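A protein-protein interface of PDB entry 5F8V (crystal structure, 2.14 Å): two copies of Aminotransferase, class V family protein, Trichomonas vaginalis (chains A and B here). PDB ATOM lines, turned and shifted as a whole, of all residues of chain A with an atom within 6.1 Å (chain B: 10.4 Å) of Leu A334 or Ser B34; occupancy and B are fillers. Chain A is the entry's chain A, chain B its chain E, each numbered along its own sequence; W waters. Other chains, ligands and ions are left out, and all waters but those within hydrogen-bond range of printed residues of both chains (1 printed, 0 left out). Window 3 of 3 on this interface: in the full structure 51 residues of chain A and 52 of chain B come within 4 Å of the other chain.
Hydrophobic or aromatic side chains of chain B within 4 Å of the printed part of chain A: Met B36. Along chain B the printed residues that touch a printed residue of chain A span positions 34 to 42. Along chain A the printed residues that touch a printed residue of chain B span positions 6 to 334. Among the printed residues, no Asp or Glu carboxylate lies within 4 Å of a Lys or Arg side-chain nitrogen of the other chain.
Of chain B, only Ser B34 (3.98 Å) and Met B36 (3.7 Å) come within 4 Å of Leu A334. Ser B34 touches just one residue of chain A: Leu A334 (3.98 Å). Of chain B, only Gly B35 comes within 4 Å of Ala A6. No residue of chain B comes within 4 Å of Thr A329. Leu A333 touches none of the printed residues of chain B. Of the printed residues of chain B, Ser A10 touches Ser B42 (3.4 Å). Of the printed residues of chain A, Glu B40 touches Asn A8. Of the printed residues of chain A, Met B36 touches Asn A8 (3.6 Å) and Leu A334 (3.7 Å). Of the printed residues of chain A, Gly B35 touches Ala A6. His B47 touches none of the printed residues of chain A. The nearest residue of chain A that does not touch Ser B34 is Ala A6 (4.1 Å). The nearest printed residue of chain A that does not touch Glu B40 is Ser A10 (4.2 Å).
Water W1 bridges OE2 of Glu B40 and ND2 of Asn A8.
No position is printed for both chains. Of the 6 pairs that touch across the chains among the printed residues, none has its exchanged pair printed and touching as well.
OD1 of Asn A8 is in hydrogen-bond range of N of Ser A10. The backbone NH (N) of Phe A9 sits at hydrogen-bond distance from the backbone carbonyl oxygen (O) of Leu A334, at 3.0 Å. N of Gly B35 sits close to ND2 of Asn B30, at 3.0 Å. O of Trp B31 is in hydrogen-bond range of OG of Ser B34 (2.7 Å). The backbone NH (N) of Trp B31 sits at hydrogen-bond distance from the backbone carbonyl oxygen (O) of Met B36 (2.8 Å). The backbone NH (N) of Ser B37 lies within hydrogen-bond range of the side-chain carboxylate (OE1) of Glu B40.
Ser A10 touches Ser B42 (OG to CB, 3.4 Å). Leu A334 touches Ser B34 (CD1 to O, 3.98 Å). Leu A334 touches Met B36 (CD1 to CE, 3.7 Å).
N of Ala A6 is in hydrogen-bond range of O of Gly B35. The side-chain sulfur (SD) of Met B36 lies close to the side-chain amide nitrogen (ND2) of Asn A8 (3.6 Å). O of Glu B40 is in hydrogen-bond range of ND2 of Asn A8 (3.0 Å).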
ATOM      1  N   ALA A   6       6.936 -26.103  32.543  1.00  0.00           N
ATOM      2  CA  ALA A   6       5.779 -25.251  32.813  1.00  0.00           C
ATOM      3  C   ALA A   6       4.671 -25.556  31.822  1.00  0.00           C
ATOM      4  O   ALA A   6       4.900 -26.197  30.798  1.00  0.00           O
ATOM      5  CB  ALA A   6       6.174 -23.788  32.734  1.00  0.00           C
ATOM      6  N   TYR A   7       3.464 -25.111  32.152  1.00  0.00           N
ATOM      7  CA  TYR A   7       2.360 -25.099  31.202  1.00  0.00           C
ATOM      8  C   TYR A   7       2.435 -23.802  30.405  1.00  0.00           C
ATOM      9  O   TYR A   7       2.112 -22.729  30.915  1.00  0.00           O
ATOM     10  CB  TYR A   7       1.023 -25.207  31.929  1.00  0.00           C
ATOM     11  CG  TYR A   7       0.842 -26.475  32.728  1.00  0.00           C
ATOM     12  CD1 TYR A   7       1.161 -27.729  32.183  1.00  0.00           C
ATOM     13  CD2 TYR A   7       0.322 -26.436  34.022  1.00  0.00           C
ATOM     14  CE1 TYR A   7       0.970 -28.896  32.905  1.00  0.00           C
ATOM     15  CE2 TYR A   7       0.131 -27.603  34.753  1.00  0.00           C
ATOM     16  CZ  TYR A   7       0.456 -28.826  34.188  1.00  0.00           C
ATOM     17  OH  TYR A   7       0.264 -29.977  34.888  1.00  0.00           O
ATOM     18  N   ASN A   8       2.855 -23.915  29.151  1.00  0.00           N
ATOM     19  CA  ASN A   8       3.256 -22.782  28.337  1.00  0.00           C
ATOM     20  C   ASN A   8       2.179 -22.420  27.307  1.00  0.00           C
ATOM     21  O   ASN A   8       1.973 -23.148  26.336  1.00  0.00           O
ATOM     22  CB  ASN A   8       4.578 -23.134  27.649  1.00  0.00           C
ATOM     23  CG  ASN A   8       5.146 -21.997  26.819  1.00  0.00           C
ATOM     24  OD1 ASN A   8       4.705 -20.856  26.901  1.00  0.00           O
ATOM     25  ND2 ASN A   8       6.138 -22.319  26.010  1.00  0.00           N
ATOM     26  N   PHE A   9       1.507 -21.289  27.527  1.00  0.00           N
ATOM     27  CA  PHE A   9       0.479 -20.813  26.612  1.00  0.00           C
ATOM     28  C   PHE A   9       0.942 -19.638  25.743  1.00  0.00           C
ATOM     29  O   PHE A   9       0.120 -18.868  25.274  1.00  0.00           O
ATOM     30  CB  PHE A   9      -0.778 -20.460  27.404  1.00  0.00           C
ATOM     31  CG  PHE A   9      -1.422 -21.638  28.067  1.00  0.00           C
ATOM     32  CD1 PHE A   9      -2.284 -22.464  27.354  1.00  0.00           C
ATOM     33  CD2 PHE A   9      -1.171 -21.927  29.397  1.00  0.00           C
ATOM     34  CE1 PHE A   9      -2.879 -23.565  27.963  1.00  0.00           C
ATOM     35  CE2 PHE A   9      -1.765 -23.019  30.010  1.00  0.00           C
ATOM     36  CZ  PHE A   9      -2.631 -23.836  29.296  1.00  0.00           C
ATOM     37  N   SER A  10       2.249 -19.511  25.499  1.00  0.00           N
ATOM     38  CA  SER A  10       2.752 -18.426  24.670  1.00  0.00           C
ATOM     39  C   SER A  10       2.205 -18.523  23.252  1.00  0.00           C
ATOM     40  O   SER A  10       2.175 -19.601  22.667  1.00  0.00           O
ATOM     41  CB  SER A  10       4.273 -18.414  24.610  1.00  0.00           C
ATOM     42  OG  SER A  10       4.702 -17.400  23.714  1.00  0.00           O
ATOM     43  N   CYS A 328      -2.907 -17.371  37.599  1.00  0.00           N
ATOM     44  CA  CYS A 328      -2.440 -18.408  36.676  1.00  0.00           C
ATOM     45  C   CYS A 328      -0.925 -18.601  36.733  1.00  0.00           C
ATOM     46  O   CYS A 328      -0.471 -19.739  36.839  1.00  0.00           O
ATOM     47  CB  CYS A 328      -2.875 -18.101  35.243  1.00  0.00           C
ATOM     48  SG  CYS A 328      -4.654 -18.162  35.021  1.00  0.00           S
ATOM     49  N   THR A 329      -0.161 -17.503  36.686  1.00  0.00           N
ATOM     50  CA  THR A 329       1.311 -17.556  36.766  1.00  0.00           C
ATOM     51  C   THR A 329       1.811 -18.244  38.047  1.00  0.00           C
ATOM     52  O   THR A 329       2.793 -18.981  38.007  1.00  0.00           O
ATOM     53  CB  THR A 329       1.950 -16.146  36.707  1.00  0.00           C
ATOM     54  OG1 THR A 329       1.462 -15.435  35.574  1.00  0.00           O
ATOM     55  CG2 THR A 329       3.472 -16.214  36.619  1.00  0.00           C
ATOM     56  N   LYS A 332       2.039 -21.853  37.629  1.00  0.00           N
ATOM     57  CA  LYS A 332       2.853 -22.202  36.453  1.00  0.00           C
ATOM     58  C   LYS A 332       2.066 -22.332  35.117  1.00  0.00           C
ATOM     59  O   LYS A 332       2.469 -23.070  34.208  1.00  0.00           O
ATOM     60  CB  LYS A 332       3.714 -23.451  36.739  1.00  0.00           C
ATOM     61  CG  LYS A 332       4.943 -23.173  37.602  1.00  0.00           C
ATOM     62  CD  LYS A 332       5.938 -24.334  37.597  1.00  0.00           C
ATOM     63  CE  LYS A 332       6.733 -24.448  36.292  1.00  0.00           C
ATOM     64  NZ  LYS A 332       7.779 -23.396  36.089  1.00  0.00           N
ATOM     65  N   LEU A 333       0.958 -21.599  35.015  1.00  0.00           N
ATOM     66  CA  LEU A 333       0.212 -21.452  33.768  1.00  0.00           C
ATOM     67  C   LEU A 333       0.712 -20.129  33.198  1.00  0.00           C
ATOM     68  O   LEU A 333       0.311 -19.068  33.657  1.00  0.00           O
ATOM     69  CB  LEU A 333      -1.296 -21.422  34.029  1.00  0.00           C
ATOM     70  CG  LEU A 333      -1.921 -22.680  34.639  1.00  0.00           C
ATOM     71  CD1 LEU A 333      -3.224 -22.350  35.345  1.00  0.00           C
ATOM     72  CD2 LEU A 333      -2.139 -23.749  33.579  1.00  0.00           C
ATOM     73  N   LEU A 334       1.624 -20.205  32.234  1.00  0.00           N
ATOM     74  CA  LEU A 334       2.399 -19.041  31.800  1.00  0.00           C
ATOM     75  C   LEU A 334       1.900 -18.426  30.493  1.00  0.00           C
ATOM     76  O   LEU A 334       1.488 -19.139  29.575  1.00  0.00           O
ATOM     77  CB  LEU A 334       3.872 -19.429  31.646  1.00  0.00           C
ATOM     78  CG  LEU A 334       4.567 -19.955  32.919  1.00  0.00           C
ATOM     79  CD1 LEU A 334       6.016 -20.302  32.615  1.00  0.00           C
ATOM     80  CD2 LEU A 334       4.490 -18.949  34.054  1.00  0.00           C
ATOM     81  N   THR A 335       1.970 -17.095  30.439  1.00  0.00           N
ATOM     82  CA  THR A 335       1.635 -16.280  29.261  1.00  0.00           C
ATOM     83  C   THR A 335       0.163 -16.412  28.865  1.00  0.00           C
ATOM     84  O   THR A 335      -0.194 -16.570  27.692  1.00  0.00           O
ATOM     85  CB  THR A 335       2.596 -16.558  28.083  1.00  0.00           C
ATOM     86  OG1 THR A 335       3.939 -16.605  28.572  1.00  0.00           O
ATOM     87  CG2 THR A 335       2.509 -15.453  27.006  1.00  0.00           C
ATOM     88  N   LEU A 336      -0.690 -16.338  29.882  1.00  0.00           N
ATOM     89  CA  LEU A 336      -2.126 -16.205  29.677  1.00  0.00           C
ATOM     90  C   LEU A 336      -2.531 -14.742  29.531  1.00  0.00           C
ATOM     91  O   LEU A 336      -3.690 -14.453  29.284  1.00  0.00           O
ATOM     92  CB  LEU A 336      -2.892 -16.903  30.808  1.00  0.00           C
ATOM     93  CG  LEU A 336      -2.925 -18.417  30.561  1.00  0.00           C
ATOM     94  CD1 LEU A 336      -2.999 -19.192  31.845  1.00  0.00           C
ATOM     95  CD2 LEU A 336      -4.079 -18.799  29.642  1.00  0.00           C
ATOM     96  N   LYS A 337      -1.569 -13.827  29.676  1.00  0.00           N
ATOM     97  CA  LYS A 337      -1.774 -12.409  29.393  1.00  0.00           C
ATOM     98  C   LYS A 337      -2.062 -12.220  27.905  1.00  0.00           C
ATOM     99  O   LYS A 337      -1.276 -12.655  27.063  1.00  0.00           O
ATOM    100  CB  LYS A 337      -0.522 -11.623  29.789  1.00  0.00           C
ATOM    101  CG  LYS A 337      -0.621 -10.118  29.629  1.00  0.00           C
ATOM    102  CD  LYS A 337       0.576  -9.428  30.267  1.00  0.00           C
ATOM    103  CE  LYS A 337       0.314  -7.949  30.505  1.00  0.00           C
ATOM    104  NZ  LYS A 337       1.415  -7.347  31.312  1.00  0.00           N
ATOM    105  N   GLU B  27      20.643 -27.432  28.518  1.00  0.00           N
ATOM    106  CA  GLU B  27      19.601 -26.420  28.749  1.00  0.00           C
ATOM    107  C   GLU B  27      18.329 -26.614  27.903  1.00  0.00           C
ATOM    108  O   GLU B  27      17.366 -25.855  28.056  1.00  0.00           O
ATOM    109  CB  GLU B  27      20.151 -25.028  28.418  1.00  0.00           C
ATOM    110  CG  GLU B  27      21.096 -24.458  29.453  1.00  0.00           C
ATOM    111  CD  GLU B  27      21.544 -23.053  29.113  1.00  0.00           C
ATOM    112  OE1 GLU B  27      21.686 -22.721  27.912  1.00  0.00           O
ATOM    113  OE2 GLU B  27      21.755 -22.274  30.061  1.00  0.00           O
ATOM    114  N   MET B  28      18.325 -27.612  27.026  1.00  0.00           N
ATOM    115  CA  MET B  28      17.356 -27.674  25.928  1.00  0.00           C
ATOM    116  C   MET B  28      15.892 -27.723  26.388  1.00  0.00           C
ATOM    117  O   MET B  28      15.059 -27.061  25.792  1.00  0.00           O
ATOM    118  CB  MET B  28      17.660 -28.866  25.006  1.00  0.00           C
ATOM    119  CG  MET B  28      16.806 -28.938  23.746  1.00  0.00           C
ATOM    120  SD  MET B  28      17.131 -27.592  22.593  1.00  0.00           S
ATOM    121  CE  MET B  28      18.618 -28.249  21.841  1.00  0.00           C
ATOM    122  N   THR B  29      15.596 -28.489  27.437  1.00  0.00           N
ATOM    123  CA  THR B  29      14.221 -28.643  27.939  1.00  0.00           C
ATOM    124  C   THR B  29      13.846 -27.593  28.999  1.00  0.00           C
ATOM    125  O   THR B  29      12.660 -27.408  29.306  1.00  0.00           O
ATOM    126  CB  THR B  29      14.000 -30.039  28.560  1.00  0.00           C
ATOM    127  OG1 THR B  29      14.754 -30.163  29.774  1.00  0.00           O
ATOM    128  CG2 THR B  29      14.419 -31.144  27.601  1.00  0.00           C
ATOM    129  N   ASN B  30      14.851 -26.930  29.569  1.00  0.00           N
ATOM    130  CA  ASN B  30      14.639 -25.997  30.663  1.00  0.00           C
ATOM    131  C   ASN B  30      15.773 -24.967  30.729  1.00  0.00           C
ATOM    132  O   ASN B  30      16.870 -25.273  31.173  1.00  0.00           O
ATOM    133  CB  ASN B  30      14.500 -26.796  31.969  1.00  0.00           C
ATOM    134  CG  ASN B  30      14.531 -25.932  33.224  1.00  0.00           C
ATOM    135  OD1 ASN B  30      15.134 -26.321  34.226  1.00  0.00           O
ATOM    136  ND2 ASN B  30      13.895 -24.776  33.189  1.00  0.00           N
ATOM    137  N   TRP B  31      15.476 -23.745  30.289  1.00  0.00           N
ATOM    138  CA  TRP B  31      16.464 -22.686  30.127  1.00  0.00           C
ATOM    139  C   TRP B  31      16.192 -21.538  31.104  1.00  0.00           C
ATOM    140  O   TRP B  31      15.041 -21.142  31.281  1.00  0.00           O
ATOM    141  CB  TRP B  31      16.396 -22.205  28.678  1.00  0.00           C
ATOM    142  CG  TRP B  31      17.115 -20.945  28.381  1.00  0.00           C
ATOM    143  CD1 TRP B  31      18.464 -20.769  28.269  1.00  0.00           C
ATOM    144  CD2 TRP B  31      16.521 -19.677  28.122  1.00  0.00           C
ATOM    145  NE1 TRP B  31      18.749 -19.463  27.964  1.00  0.00           N
ATOM    146  CE2 TRP B  31      17.571 -18.769  27.869  1.00  0.00           C
ATOM    147  CE3 TRP B  31      15.202 -19.216  28.085  1.00  0.00           C
ATOM    148  CZ2 TRP B  31      17.338 -17.420  27.576  1.00  0.00           C
ATOM    149  CZ3 TRP B  31      14.970 -17.880  27.801  1.00  0.00           C
ATOM    150  CH2 TRP B  31      16.034 -16.996  27.553  1.00  0.00           C
ATOM    151  N   ARG B  32      17.246 -21.007  31.727  1.00  0.00           N
ATOM    152  CA  ARG B  32      17.132 -19.912  32.723  1.00  0.00           C
ATOM    153  C   ARG B  32      16.180 -20.273  33.882  1.00  0.00           C
ATOM    154  O   ARG B  32      15.532 -19.402  34.468  1.00  0.00           O
ATOM    155  CB  ARG B  32      16.703 -18.586  32.046  1.00  0.00           C
ATOM    156  CG  ARG B  32      17.810 -17.565  31.829  1.00  0.00           C
ATOM    157  CD  ARG B  32      17.252 -16.323  31.137  1.00  0.00           C
ATOM    158  NE  ARG B  32      18.162 -15.168  31.136  1.00  0.00           N
ATOM    159  CZ  ARG B  32      19.262 -15.043  30.388  1.00  0.00           C
ATOM    160  NH1 ARG B  32      19.651 -16.015  29.566  1.00  0.00           N
ATOM    161  NH2 ARG B  32      20.000 -13.936  30.473  1.00  0.00           N
ATOM    162  N   ASN B  33      16.109 -21.560  34.208  1.00  0.00           N
ATOM    163  CA  ASN B  33      15.142 -22.074  35.173  1.00  0.00           C
ATOM    164  C   ASN B  33      13.688 -21.612  34.892  1.00  0.00           C
ATOM    165  O   ASN B  33      12.947 -21.270  35.813  1.00  0.00           O
ATOM    166  CB  ASN B  33      15.592 -21.694  36.597  1.00  0.00           C
ATOM    167  CG  ASN B  33      14.986 -22.585  37.663  1.00  0.00           C
ATOM    168  OD1 ASN B  33      14.403 -22.097  38.635  1.00  0.00           O
ATOM    169  ND2 ASN B  33      15.119 -23.900  37.488  1.00  0.00           N
ATOM    170  N   SER B  34      13.292 -21.615  33.613  1.00  0.00           N
ATOM    171  CA  SER B  34      11.999 -21.054  33.178  1.00  0.00           C
ATOM    172  C   SER B  34      10.878 -22.082  33.022  1.00  0.00           C
ATOM    173  O   SER B  34       9.731 -21.715  32.795  1.00  0.00           O
ATOM    174  CB  SER B  34      12.166 -20.309  31.847  1.00  0.00           C
ATOM    175  OG  SER B  34      12.423 -21.202  30.767  1.00  0.00           O
ATOM    176  N   GLY B  35      11.199 -23.357  33.192  1.00  0.00           N
ATOM    177  CA  GLY B  35      10.362 -24.459  32.738  1.00  0.00           C
ATOM    178  C   GLY B  35      10.091 -24.566  31.235  1.00  0.00           C
ATOM    179  O   GLY B  35       9.121 -25.229  30.837  1.00  0.00           O
ATOM    180  N   MET B  36      10.930 -23.935  30.409  1.00  0.00           N
ATOM    181  CA  MET B  36      10.753 -23.904  28.948  1.00  0.00           C
ATOM    182  C   MET B  36      12.113 -23.940  28.243  1.00  0.00           C
ATOM    183  O   MET B  36      13.098 -23.441  28.770  1.00  0.00           O
ATOM    184  CB  MET B  36      10.016 -22.619  28.522  1.00  0.00           C
ATOM    185  CG  MET B  36       8.580 -22.491  29.042  1.00  0.00           C
ATOM    186  SD  MET B  36       7.874 -20.844  28.820  1.00  0.00           S
ATOM    187  CE  MET B  36       8.674 -19.922  30.130  1.00  0.00           C
ATOM    188  N   SER B  37      12.148 -24.505  27.036  1.00  0.00           N
ATOM    189  CA  SER B  37      13.270 -24.317  26.121  1.00  0.00           C
ATOM    190  C   SER B  37      13.367 -22.842  25.739  1.00  0.00           C
ATOM    191  O   SER B  37      12.357 -22.146  25.705  1.00  0.00           O
ATOM    192  CB  SER B  37      13.061 -25.141  24.842  1.00  0.00           C
ATOM    193  OG  SER B  37      14.221 -25.166  24.020  1.00  0.00           O
ATOM    194  N   VAL B  38      14.573 -22.374  25.429  1.00  0.00           N
ATOM    195  CA  VAL B  38      14.753 -21.059  24.790  1.00  0.00           C
ATOM    196  C   VAL B  38      13.959 -20.977  23.463  1.00  0.00           C
ATOM    197  O   VAL B  38      13.518 -19.905  23.066  1.00  0.00           O
ATOM    198  CB  VAL B  38      16.251 -20.728  24.561  1.00  0.00           C
ATOM    199  CG1 VAL B  38      16.871 -21.614  23.479  1.00  0.00           C
ATOM    200  CG2 VAL B  38      16.430 -19.248  24.219  1.00  0.00           C
ATOM    201  N   ILE B  39      13.771 -22.125  22.816  1.00  0.00           N
ATOM    202  CA  ILE B  39      12.929 -22.275  21.617  1.00  0.00           C
ATOM    203  C   ILE B  39      11.446 -21.924  21.854  1.00  0.00           C
ATOM    204  O   ILE B  39      10.765 -21.508  20.923  1.00  0.00           O
ATOM    205  CB  ILE B  39      13.041 -23.729  21.059  1.00  0.00           C
ATOM    206  CG1 ILE B  39      14.451 -23.983  20.517  1.00  0.00           C
ATOM    207  CG2 ILE B  39      12.013 -24.020  19.963  1.00  0.00           C
ATOM    208  CD1 ILE B  39      14.825 -25.453  20.444  1.00  0.00           C
ATOM    209  N   GLU B  40      10.955 -22.095  23.085  1.00  0.00           N
ATOM    210  CA  GLU B  40       9.512 -22.022  23.390  1.00  0.00           C
ATOM    211  C   GLU B  40       9.033 -20.720  24.052  1.00  0.00           C
ATOM    212  O   GLU B  40       7.841 -20.561  24.318  1.00  0.00           O
ATOM    213  CB  GLU B  40       9.142 -23.197  24.288  1.00  0.00           C
ATOM    214  CG  GLU B  40       9.404 -24.559  23.674  1.00  0.00           C
ATOM    215  CD  GLU B  40       9.210 -25.671  24.677  1.00  0.00           C
ATOM    216  OE1 GLU B  40       9.989 -25.727  25.658  1.00  0.00           O
ATOM    217  OE2 GLU B  40       8.267 -26.475  24.499  1.00  0.00           O
ATOM    218  N   VAL B  41       9.951 -19.784  24.273  1.00  0.00           N
ATOM    219  CA  VAL B  41       9.708 -18.628  25.119  1.00  0.00           C
ATOM    220  C   VAL B  41       9.272 -17.427  24.265  1.00  0.00           C
ATOM    221  O   VAL B  41       9.778 -17.229  23.142  1.00  0.00           O
ATOM    222  CB  VAL B  41      10.980 -18.359  25.981  1.00  0.00           C
ATOM    223  CG1 VAL B  41      12.037 -17.552  25.232  1.00  0.00           C
ATOM    224  CG2 VAL B  41      10.632 -17.724  27.317  1.00  0.00           C
ATOM    225  N   SER B  42       8.308 -16.651  24.776  1.00  0.00           N
ATOM    226  CA  SER B  42       7.849 -15.443  24.087  1.00  0.00           C
ATOM    227  C   SER B  42       8.995 -14.443  23.985  1.00  0.00           C
ATOM    228  O   SER B  42       9.790 -14.303  24.906  1.00  0.00           O
ATOM    229  CB  SER B  42       6.658 -14.794  24.804  1.00  0.00           C
ATOM    230  OG  SER B  42       6.321 -13.540  24.219  1.00  0.00           O
ATOM    231  N   GLY B  45       8.514 -11.467  26.335  1.00  0.00           N
ATOM    232  CA  GLY B  45       8.623 -11.803  27.749  1.00  0.00           C
ATOM    233  C   GLY B  45       9.919 -11.308  28.355  1.00  0.00           C
ATOM    234  O   GLY B  45      10.837 -10.878  27.639  1.00  0.00           O
ATOM    235  N   LYS B  46       9.999 -11.397  29.682  1.00  0.00           N
ATOM    236  CA  LYS B  46      11.124 -10.858  30.439  1.00  0.00           C
ATOM    237  C   LYS B  46      12.416 -11.600  30.109  1.00  0.00           C
ATOM    238  O   LYS B  46      13.430 -10.980  29.795  1.00  0.00           O
ATOM    239  CB  LYS B  46      10.832 -10.946  31.939  1.00  0.00           C
ATOM    240  CG  LYS B  46      11.854 -10.249  32.834  1.00  0.00           C
ATOM    241  CD  LYS B  46      11.419 -10.231  34.298  1.00  0.00           C
ATOM    242  CE  LYS B  46      11.497 -11.610  34.942  1.00  0.00           C
ATOM    243  NZ  LYS B  46      10.972 -11.608  36.339  1.00  0.00           N
ATOM    244  N   HIS B  47      12.347 -12.929  30.162  1.00  0.00           N
ATOM    245  CA  HIS B  47      13.502 -13.805  29.950  1.00  0.00           C
ATOM    246  C   HIS B  47      14.194 -13.551  28.610  1.00  0.00           C
ATOM    247  O   HIS B  47      15.420 -13.404  28.568  1.00  0.00           O
ATOM    248  CB  HIS B  47      13.084 -15.279  30.031  1.00  0.00           C
ATOM    249  CG  HIS B  47      12.681 -15.721  31.404  1.00  0.00           C
ATOM    250  ND1 HIS B  47      13.537 -15.672  32.480  1.00  0.00           N
ATOM    251  CD2 HIS B  47      11.522 -16.244  31.868  1.00  0.00           C
ATOM    252  CE1 HIS B  47      12.918 -16.130  33.554  1.00  0.00           C
ATOM    253  NE2 HIS B  47      11.694 -16.481  33.210  1.00  0.00           N
ATOM    254  N   TRP B  48      13.422 -13.491  27.521  1.00  0.00           N
ATOM    255  CA  TRP B  48      14.034 -13.253  26.207  1.00  0.00           C
ATOM    256  C   TRP B  48      14.615 -11.842  26.082  1.00  0.00           C
ATOM    257  O   TRP B  48      15.728 -11.674  25.583  1.00  0.00           O
ATOM    258  CB  TRP B  48      13.111 -13.534  25.007  1.00  0.00           C
ATOM    259  CG  TRP B  48      13.900 -13.197  23.794  1.00  0.00           C
ATOM    260  CD1 TRP B  48      13.791 -12.073  23.022  1.00  0.00           C
ATOM    261  CD2 TRP B  48      15.063 -13.886  23.332  1.00  0.00           C
ATOM    262  NE1 TRP B  48      14.773 -12.063  22.066  1.00  0.00           N
ATOM    263  CE2 TRP B  48      15.566 -13.165  22.232  1.00  0.00           C
ATOM    264  CE3 TRP B  48      15.707 -15.062  23.720  1.00  0.00           C
ATOM    265  CZ2 TRP B  48      16.676 -13.590  21.507  1.00  0.00           C
ATOM    266  CZ3 TRP B  48      16.809 -15.486  23.000  1.00  0.00           C
ATOM    267  CH2 TRP B  48      17.286 -14.745  21.910  1.00  0.00           C
ATOM    268  N   GLU B  50      15.851  -9.970  28.338  1.00  0.00           N
ATOM    269  CA  GLU B  50      17.148 -10.006  29.038  1.00  0.00           C
ATOM    270  C   GLU B  50      18.251 -10.621  28.176  1.00  0.00           C
ATOM    271  O   GLU B  50      19.341 -10.059  28.056  1.00  0.00           O
ATOM    272  CB  GLU B  50      17.063 -10.810  30.340  1.00  0.00           C
ATOM    273  CG  GLU B  50      16.390 -10.103  31.502  1.00  0.00           C
ATOM    274  CD  GLU B  50      16.514 -10.898  32.792  1.00  0.00           C
ATOM    275  OE1 GLU B  50      17.291 -10.485  33.679  1.00  0.00           O
ATOM    276  OE2 GLU B  50      15.854 -11.953  32.911  1.00  0.00           O
ATOM    277  N   TYR B 252      20.606 -16.498  20.996  1.00  0.00           N
ATOM    278  CA  TYR B 252      20.980 -17.299  22.170  1.00  0.00           C
ATOM    279  C   TYR B 252      22.308 -18.044  21.987  1.00  0.00           C
ATOM    280  O   TYR B 252      23.192 -17.991  22.858  1.00  0.00           O
ATOM    281  CB  TYR B 252      19.848 -18.289  22.501  1.00  0.00           C
ATOM    282  CG  TYR B 252      20.246 -19.539  23.257  1.00  0.00           C
ATOM    283  CD1 TYR B 252      20.542 -20.724  22.577  1.00  0.00           C
ATOM    284  CD2 TYR B 252      20.292 -19.551  24.653  1.00  0.00           C
ATOM    285  CE1 TYR B 252      20.893 -21.879  23.268  1.00  0.00           C
ATOM    286  CE2 TYR B 252      20.635 -20.698  25.347  1.00  0.00           C
ATOM    287  CZ  TYR B 252      20.934 -21.860  24.654  1.00  0.00           C
ATOM    288  OH  TYR B 252      21.278 -23.008  25.341  1.00  0.00           O
HETATM  289  O   HOH W   1       6.635 -25.154  26.460  1.00  0.00           O
